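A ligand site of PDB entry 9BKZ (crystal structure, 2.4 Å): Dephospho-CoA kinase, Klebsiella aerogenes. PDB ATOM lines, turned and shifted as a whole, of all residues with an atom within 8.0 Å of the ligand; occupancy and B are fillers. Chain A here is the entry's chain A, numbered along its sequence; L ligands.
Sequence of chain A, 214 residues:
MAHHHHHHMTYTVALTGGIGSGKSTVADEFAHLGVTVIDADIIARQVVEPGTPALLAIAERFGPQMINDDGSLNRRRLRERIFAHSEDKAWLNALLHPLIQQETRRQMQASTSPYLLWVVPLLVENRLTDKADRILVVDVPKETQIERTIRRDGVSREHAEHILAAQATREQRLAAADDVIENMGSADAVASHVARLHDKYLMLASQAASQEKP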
ATOM      1  N   ARG A  45     -29.012   2.355 -24.724  1.00  0.00           N
ATOM      2  CA  ARG A  45     -27.770   2.961 -24.274  1.00  0.00           C
ATOM      3  C   ARG A  45     -27.564   4.339 -24.889  1.00  0.00           C
ATOM      4  O   ARG A  45     -26.828   5.154 -24.314  1.00  0.00           O
ATOM      5  CB  ARG A  45     -26.590   2.057 -24.616  1.00  0.00           C
ATOM      6  CG  ARG A  45     -26.752   0.632 -24.083  1.00  0.00           C
ATOM      7  CD  ARG A  45     -25.422   0.015 -23.678  1.00  0.00           C
ATOM      8  NE  ARG A  45     -25.632  -1.153 -22.819  1.00  0.00           N
ATOM      9  CZ  ARG A  45     -24.733  -1.639 -21.977  1.00  0.00           C
ATOM     10  NH1 ARG A  45     -23.527  -1.091 -21.864  1.00  0.00           N
ATOM     11  NH2 ARG A  45     -25.042  -2.688 -21.233  1.00  0.00           N
ATOM     12  N   PRO A  64     -25.589  13.232  -8.485  1.00  0.00           N
ATOM     13  CA  PRO A  64     -24.561  13.342  -9.526  1.00  0.00           C
ATOM     14  C   PRO A  64     -23.621  12.155  -9.602  1.00  0.00           C
ATOM     15  O   PRO A  64     -22.897  12.021 -10.595  1.00  0.00           O
ATOM     16  CB  PRO A  64     -23.808  14.619  -9.149  1.00  0.00           C
ATOM     17  CG  PRO A  64     -24.025  14.764  -7.671  1.00  0.00           C
ATOM     18  CD  PRO A  64     -25.405  14.215  -7.406  1.00  0.00           C
ATOM     19  N   GLN A  65     -23.600  11.280  -8.580  1.00  0.00           N
ATOM     20  CA  GLN A  65     -22.709  10.129  -8.624  1.00  0.00           C
ATOM     21  C   GLN A  65     -23.125   9.106  -9.682  1.00  0.00           C
ATOM     22  O   GLN A  65     -22.374   8.155  -9.916  1.00  0.00           O
ATOM     23  CB  GLN A  65     -22.635   9.469  -7.245  1.00  0.00           C
ATOM     24  CG  GLN A  65     -23.908   8.768  -6.788  1.00  0.00           C
ATOM     25  CD  GLN A  65     -24.976   9.741  -6.309  1.00  0.00           C
ATOM     26  OE1 GLN A  65     -24.752  10.949  -6.252  1.00  0.00           O
ATOM     27  NE2 GLN A  65     -26.139   9.207  -5.956  1.00  0.00           N
ATOM     28  N   MET A  66     -24.283   9.266 -10.297  1.00  0.00           N
ATOM     29  CA  MET A  66     -24.698   8.403 -11.397  1.00  0.00           C
ATOM     30  C   MET A  66     -24.026   8.766 -12.707  1.00  0.00           C
ATOM     31  O   MET A  66     -24.291   8.100 -13.726  1.00  0.00           O
ATOM     32  CB  MET A  66     -26.219   8.464 -11.554  1.00  0.00           C
ATOM     33  CG  MET A  66     -26.986   7.935 -10.356  1.00  0.00           C
ATOM     34  SD  MET A  66     -26.993   6.130 -10.316  1.00  0.00           S
ATOM     35  CE  MET A  66     -27.348   5.842  -8.587  1.00  0.00           C
ATOM     36  N   ILE A  67     -23.182   9.793 -12.713  1.00  0.00           N
ATOM     37  CA  ILE A  67     -22.453  10.230 -13.902  1.00  0.00           C
ATOM     38  C   ILE A  67     -20.978  10.123 -13.590  1.00  0.00           C
ATOM     39  O   ILE A  67     -20.504  10.700 -12.600  1.00  0.00           O
ATOM     40  CB  ILE A  67     -22.837  11.660 -14.299  1.00  0.00           C
ATOM     41  CG1 ILE A  67     -24.357  11.763 -14.491  1.00  0.00           C
ATOM     42  CG2 ILE A  67     -22.113  12.067 -15.584  1.00  0.00           C
ATOM     43  CD1 ILE A  67     -24.859  13.170 -14.777  1.00  0.00           C
ATOM     44  N   ASN A  68     -20.237   9.404 -14.431  1.00  0.00           N
ATOM     45  CA  ASN A  68     -18.835   9.116 -14.148  1.00  0.00           C
ATOM     46  C   ASN A  68     -17.948  10.221 -14.709  1.00  0.00           C
ATOM     47  O   ASN A  68     -18.426  11.281 -15.125  1.00  0.00           O
ATOM     48  CB  ASN A  68     -18.474   7.730 -14.697  1.00  0.00           C
ATOM     49  CG  ASN A  68     -18.819   7.577 -16.170  1.00  0.00           C
ATOM     50  OD1 ASN A  68     -18.903   8.554 -16.911  1.00  0.00           O
ATOM     51  ND2 ASN A  68     -19.022   6.333 -16.592  1.00  0.00           N
ATOM     52  N   ASP A  69     -16.631   9.973 -14.736  1.00  0.00           N
ATOM     53  CA  ASP A  69     -15.671  11.019 -15.078  1.00  0.00           C
ATOM     54  C   ASP A  69     -15.773  11.455 -16.532  1.00  0.00           C
ATOM     55  O   ASP A  69     -15.351  12.567 -16.861  1.00  0.00           O
ATOM     56  CB  ASP A  69     -14.252  10.540 -14.784  1.00  0.00           C
ATOM     57  CG  ASP A  69     -13.965  10.468 -13.293  1.00  0.00           C
ATOM     58  OD1 ASP A  69     -14.781  10.983 -12.503  1.00  0.00           O
ATOM     59  OD2 ASP A  69     -12.925   9.896 -12.918  1.00  0.00           O
ATOM     60  N   ASP A  70     -16.293  10.601 -17.420  1.00  0.00           N
ATOM     61  CA  ASP A  70     -16.453  10.959 -18.819  1.00  0.00           C
ATOM     62  C   ASP A  70     -17.899  11.313 -19.163  1.00  0.00           C
ATOM     63  O   ASP A  70     -18.277  11.310 -20.335  1.00  0.00           O
ATOM     64  CB  ASP A  70     -15.960   9.813 -19.713  1.00  0.00           C
ATOM     65  CG  ASP A  70     -16.812   8.576 -19.595  1.00  0.00           C
ATOM     66  OD1 ASP A  70     -17.338   8.114 -20.627  1.00  0.00           O
ATOM     67  OD2 ASP A  70     -16.968   8.060 -18.467  1.00  0.00           O
ATOM     68  N   GLY A  71     -18.701  11.647 -18.152  1.00  0.00           N
ATOM     69  CA  GLY A  71     -20.060  12.109 -18.387  1.00  0.00           C
ATOM     70  C   GLY A  71     -21.048  11.058 -18.816  1.00  0.00           C
ATOM     71  O   GLY A  71     -22.095  11.402 -19.362  1.00  0.00           O
ATOM     72  N   SER A  72     -20.751   9.782 -18.560  1.00  0.00           N
ATOM     73  CA  SER A  72     -21.626   8.690 -18.960  1.00  0.00           C
ATOM     74  C   SER A  72     -22.223   8.008 -17.739  1.00  0.00           C
ATOM     75  O   SER A  72     -21.749   8.181 -16.606  1.00  0.00           O
ATOM     76  CB  SER A  72     -20.855   7.659 -19.799  1.00  0.00           C
ATOM     77  OG  SER A  72     -19.860   7.008 -19.034  1.00  0.00           O
ATOM     78  N   LEU A  73     -23.278   7.233 -17.974  1.00  0.00           N
ATOM     79  CA  LEU A  73     -24.009   6.610 -16.889  1.00  0.00           C
ATOM     80  C   LEU A  73     -23.152   5.617 -16.132  1.00  0.00           C
ATOM     81  O   LEU A  73     -22.500   4.757 -16.736  1.00  0.00           O
ATOM     82  CB  LEU A  73     -25.251   5.917 -17.441  1.00  0.00           C
ATOM     83  CG  LEU A  73     -26.093   5.110 -16.449  1.00  0.00           C
ATOM     84  CD1 LEU A  73     -26.569   5.987 -15.311  1.00  0.00           C
ATOM     85  CD2 LEU A  73     -27.265   4.469 -17.180  1.00  0.00           C
ATOM     86  N   ASN A  74     -23.151   5.725 -14.804  1.00  0.00           N
ATOM     87  CA  ASN A  74     -22.475   4.748 -13.943  1.00  0.00           C
ATOM     88  C   ASN A  74     -23.466   3.616 -13.713  1.00  0.00           C
ATOM     89  O   ASN A  74     -24.312   3.666 -12.809  1.00  0.00           O
ATOM     90  CB  ASN A  74     -22.023   5.382 -12.644  1.00  0.00           C
ATOM     91  CG  ASN A  74     -21.150   4.454 -11.818  1.00  0.00           C
ATOM     92  OD1 ASN A  74     -21.308   3.237 -11.852  1.00  0.00           O
ATOM     93  ND2 ASN A  74     -20.213   5.033 -11.063  1.00  0.00           N
ATOM     94  N   ARG A  75     -23.373   2.576 -14.542  1.00  0.00           N
ATOM     95  CA  ARG A  75     -24.322   1.468 -14.464  1.00  0.00           C
ATOM     96  C   ARG A  75     -24.119   0.615 -13.218  1.00  0.00           C
ATOM     97  O   ARG A  75     -25.043  -0.070 -12.794  1.00  0.00           O
ATOM     98  CB  ARG A  75     -24.233   0.604 -15.718  1.00  0.00           C
ATOM     99  CG  ARG A  75     -25.052   1.140 -16.881  1.00  0.00           C
ATOM    100  CD  ARG A  75     -24.754   0.415 -18.174  1.00  0.00           C
ATOM    101  NE  ARG A  75     -24.444   1.349 -19.251  1.00  0.00           N
ATOM    102  CZ  ARG A  75     -25.351   1.957 -20.005  1.00  0.00           C
ATOM    103  NH1 ARG A  75     -26.644   1.714 -19.871  1.00  0.00           N
ATOM    104  NH2 ARG A  75     -24.947   2.818 -20.934  1.00  0.00           N
ATOM    105  N   ARG A  76     -22.921   0.642 -12.624  1.00  0.00           N
ATOM    106  CA  ARG A  76     -22.710  -0.059 -11.361  1.00  0.00           C
ATOM    107  C   ARG A  76     -23.611   0.514 -10.283  1.00  0.00           C
ATOM    108  O   ARG A  76     -24.364  -0.223  -9.622  1.00  0.00           O
ATOM    109  CB  ARG A  76     -21.236   0.040 -10.952  1.00  0.00           C
ATOM    110  CG  ARG A  76     -20.792  -1.025  -9.969  1.00  0.00           C
ATOM    111  CD  ARG A  76     -19.376  -0.763  -9.482  1.00  0.00           C
ATOM    112  NE  ARG A  76     -19.314   0.403  -8.613  1.00  0.00           N
ATOM    113  CZ  ARG A  76     -18.189   0.878  -8.074  1.00  0.00           C
ATOM    114  NH1 ARG A  76     -17.017   0.315  -8.309  1.00  0.00           N
ATOM    115  NH2 ARG A  76     -18.260   1.949  -7.287  1.00  0.00           N
ATOM    116  N   ARG A  77     -23.563   1.833 -10.078  1.00  0.00           N
ATOM    117  CA  ARG A  77     -24.373   2.460  -9.049  1.00  0.00           C
ATOM    118  C   ARG A  77     -25.865   2.371  -9.373  1.00  0.00           C
ATOM    119  O   ARG A  77     -26.679   2.232  -8.460  1.00  0.00           O
ATOM    120  CB  ARG A  77     -23.949   3.908  -8.862  1.00  0.00           C
ATOM    121  CG  ARG A  77     -22.769   4.058  -7.910  1.00  0.00           C
ATOM    122  CD  ARG A  77     -21.978   5.333  -8.144  1.00  0.00           C
ATOM    123  NE  ARG A  77     -20.686   5.270  -7.472  1.00  0.00           N
ATOM    124  CZ  ARG A  77     -19.747   6.195  -7.559  1.00  0.00           C
ATOM    125  NH1 ARG A  77     -19.917   7.289  -8.267  1.00  0.00           N
ATOM    126  NH2 ARG A  77     -18.600   6.015  -6.909  1.00  0.00           N
ATOM    127  N   LEU A  78     -26.226   2.438 -10.651  1.00  0.00           N
ATOM    128  CA  LEU A  78     -27.638   2.298 -11.005  1.00  0.00           C
ATOM    129  C   LEU A  78     -28.139   0.887 -10.692  1.00  0.00           C
ATOM    130  O   LEU A  78     -29.226   0.726 -10.144  1.00  0.00           O
ATOM    131  CB  LEU A  78     -27.842   2.627 -12.478  1.00  0.00           C
ATOM    132  CG  LEU A  78     -29.296   2.728 -12.950  1.00  0.00           C
ATOM    133  CD1 LEU A  78     -30.056   3.801 -12.202  1.00  0.00           C
ATOM    134  CD2 LEU A  78     -29.332   3.003 -14.453  1.00  0.00           C
ATOM    135  N   ARG A  79     -27.347  -0.131 -11.029  1.00  0.00           N
ATOM    136  CA  ARG A  79     -27.696  -1.502 -10.643  1.00  0.00           C
ATOM    137  C   ARG A  79     -27.914  -1.601  -9.142  1.00  0.00           C
ATOM    138  O   ARG A  79     -28.944  -2.113  -8.674  1.00  0.00           O
ATOM    139  CB  ARG A  79     -26.606  -2.481 -11.093  1.00  0.00           C
ATOM    140  CG  ARG A  79     -26.773  -2.982 -12.512  1.00  0.00           C
ATOM    141  CD  ARG A  79     -25.803  -4.134 -12.813  1.00  0.00           C
ATOM    142  NE  ARG A  79     -24.430  -3.674 -12.998  1.00  0.00           N
ATOM    143  CZ  ARG A  79     -23.908  -3.306 -14.165  1.00  0.00           C
ATOM    144  NH1 ARG A  79     -24.623  -3.311 -15.275  1.00  0.00           N
ATOM    145  NH2 ARG A  79     -22.641  -2.909 -14.207  1.00  0.00           N
ATOM    146  N   GLU A  80     -26.946  -1.102  -8.357  1.00  0.00           N
ATOM    147  CA  GLU A  80     -27.072  -1.156  -6.901  1.00  0.00           C
ATOM    148  C   GLU A  80     -28.337  -0.449  -6.430  1.00  0.00           C
ATOM    149  O   GLU A  80     -29.094  -0.984  -5.625  1.00  0.00           O
ATOM    150  CB  GLU A  80     -25.831  -0.525  -6.258  1.00  0.00           C
ATOM    151  CG  GLU A  80     -24.557  -1.318  -6.486  1.00  0.00           C
ATOM    152  CD  GLU A  80     -23.307  -0.532  -6.166  1.00  0.00           C
ATOM    153  OE1 GLU A  80     -23.412   0.684  -5.919  1.00  0.00           O
ATOM    154  OE2 GLU A  80     -22.206  -1.134  -6.166  1.00  0.00           O
HETATM  155  N1  LIG L   1     -20.136   0.642 -15.133  1.00  0.00           N
HETATM  156  C1  LIG L   1     -19.435   0.143 -14.115  1.00  0.00           C
HETATM  157  N2  LIG L   1     -18.636   0.763 -13.244  1.00  0.00           N
HETATM  158  C2  LIG L   1     -18.588   2.063 -13.511  1.00  0.00           C
HETATM  159  C3  LIG L   1     -19.241   2.743 -14.517  1.00  0.00           C
HETATM  160  C4  LIG L   1     -20.055   1.972 -15.373  1.00  0.00           C
HETATM  161  N3  LIG L   1     -20.741   2.488 -16.385  1.00  0.00           N
HETATM  162  N4  LIG L   1     -18.941   4.096 -14.469  1.00  0.00           N
HETATM  163  C5  LIG L   1     -18.121   4.207 -13.450  1.00  0.00           C
HETATM  164  N5  LIG L   1     -17.874   3.013 -12.837  1.00  0.00           N
HETATM  165  C6  LIG L   1     -17.039   2.777 -11.679  1.00  0.00           C
HETATM  166  C7  LIG L   1     -15.653   3.416 -11.813  1.00  0.00           C
HETATM  167  O1  LIG L   1     -14.707   2.494 -12.317  1.00  0.00           O
HETATM  168  C8  LIG L   1     -15.365   3.810 -10.368  1.00  0.00           C
HETATM  169  O2  LIG L   1     -14.955   2.685  -9.619  1.00  0.00           O
HETATM  170  P1  LIG L   1     -13.647   3.056  -8.760  1.00  0.00           P
HETATM  171  O3  LIG L   1     -13.998   4.281  -7.936  1.00  0.00           O
HETATM  172  O4  LIG L   1     -13.347   1.856  -7.894  1.00  0.00           O
HETATM  173  O5  LIG L   1     -12.555   3.328  -9.760  1.00  0.00           O
HETATM  174  C9  LIG L   1     -16.728   4.273  -9.903  1.00  0.00           C
HETATM  175  O6  LIG L   1     -17.659   3.379 -10.570  1.00  0.00           O
HETATM  176  C10 LIG L   1     -17.078   5.699 -10.248  1.00  0.00           C
HETATM  177  O7  LIG L   1     -15.892   6.408 -10.668  1.00  0.00           O
HETATM  178  P2  LIG L   1     -16.079   7.783 -11.461  1.00  0.00           P
HETATM  179  O8  LIG L   1     -17.429   8.341 -11.175  1.00  0.00           O
HETATM  180  O9  LIG L   1     -15.675   7.591 -12.881  1.00  0.00           O
HETATM  181  O10 LIG L   1     -14.972   8.675 -10.730  1.00  0.00           O
HETATM  182  P3  LIG L   1     -14.926   9.366  -9.297  1.00  0.00           P
HETATM  183  O11 LIG L   1     -15.980   8.749  -8.430  1.00  0.00           O
HETATM  184  O12 LIG L   1     -14.896  10.849  -9.462  1.00  0.00           O
HETATM  185  O13 LIG L   1     -13.497   8.881  -8.781  1.00  0.00           O
HETATM  186  C11 LIG L   1     -11.148   8.531  -9.163  1.00  0.00           C
HETATM  187  C12 LIG L   1     -12.312   9.499  -9.341  1.00  0.00           C
HETATM  188  C13 LIG L   1     -11.494   7.211  -9.855  1.00  0.00           C
HETATM  189  C14 LIG L   1      -9.905   9.115  -9.836  1.00  0.00           C
HETATM  190  C15 LIG L   1     -10.843   8.294  -7.679  1.00  0.00           C
HETATM  191  O14 LIG L   1     -11.784   9.019  -6.907  1.00  0.00           O
HETATM  192  C16 LIG L   1     -10.837   6.838  -7.257  1.00  0.00           C
HETATM  193  O15 LIG L   1     -11.865   6.327  -6.814  1.00  0.00           O
HETATM  194  N6  LIG L   1      -9.694   6.183  -7.351  1.00  0.00           N
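The backbone carbonyl oxygen (O) of Leu 73 is in hydrogen-bond range of a nitrogen (N3) of the ligand (2.9 Å). An oxygen (O9) of the ligand is in hydrogen-bond range of the backbone NH (N) of Asp 69 (3.2 Å). An oxygen (O12) of the ligand sits close to the side-chain carboxylate of Asp 69, at 3.0 Å. The side-chain amide nitrogen (ND2) of Asn 74 sits at hydrogen-bond distance from an oxygen (O6) of the ligand, 3.1 Å away. A nitrogen (N4) of the ligand lies within hydrogen-bond range of the side-chain amide nitrogen (ND2) of Asn 68, 3.1 Å away. An oxygen (O2) of the ligand sits at hydrogen-bond distance from the guanidinium group (NH1) of Arg 76 (3.4 Å). The guanidinium group of Arg 77 lies within salt-bridge range of an oxygen (O8) of the ligand (3.97 Å).
The side-chain amide oxygen (OD1) of Asn 74 lies within hydrogen-bond range of the backbone NH (N) of Arg 76, at 3.2 Å. N of Arg 77 is in hydrogen-bond range of OD1 of Asn 74, 3.2 Å away. The backbone carbonyl oxygen (O) of Met 66 lies within hydrogen-bond range of the backbone NH (N) of Asn 74 (2.8 Å). The side-chain hydroxyl of Ser 72 sits at hydrogen-bond distance from the side-chain amide nitrogen of Asn 68 (2.7 Å). The side-chain amide oxygen (OD1) of Asn 68 sits close to the side-chain carboxylate (OD2) of Asp 70. The side-chain amide oxygen (OD1) of Asn 68 lies within hydrogen-bond range of the backbone NH (N) of Gly 71 (3.3 Å). The guanidinium group (NH1) of Arg 77 sits at hydrogen-bond distance from the backbone carbonyl oxygen (O) of Gln 65 (3.1 Å).
N of Arg 75 lies close to N3 of the ligand (3.2 Å). Seven residues have an atom within 4 Å of the ligand: Asn 68, Asp 69, Leu 73, Asn 74, Arg 75, Arg 76 and Arg 77. The nearest printed residue that does not touch the ligand is Ile 67 (4.1 Å).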
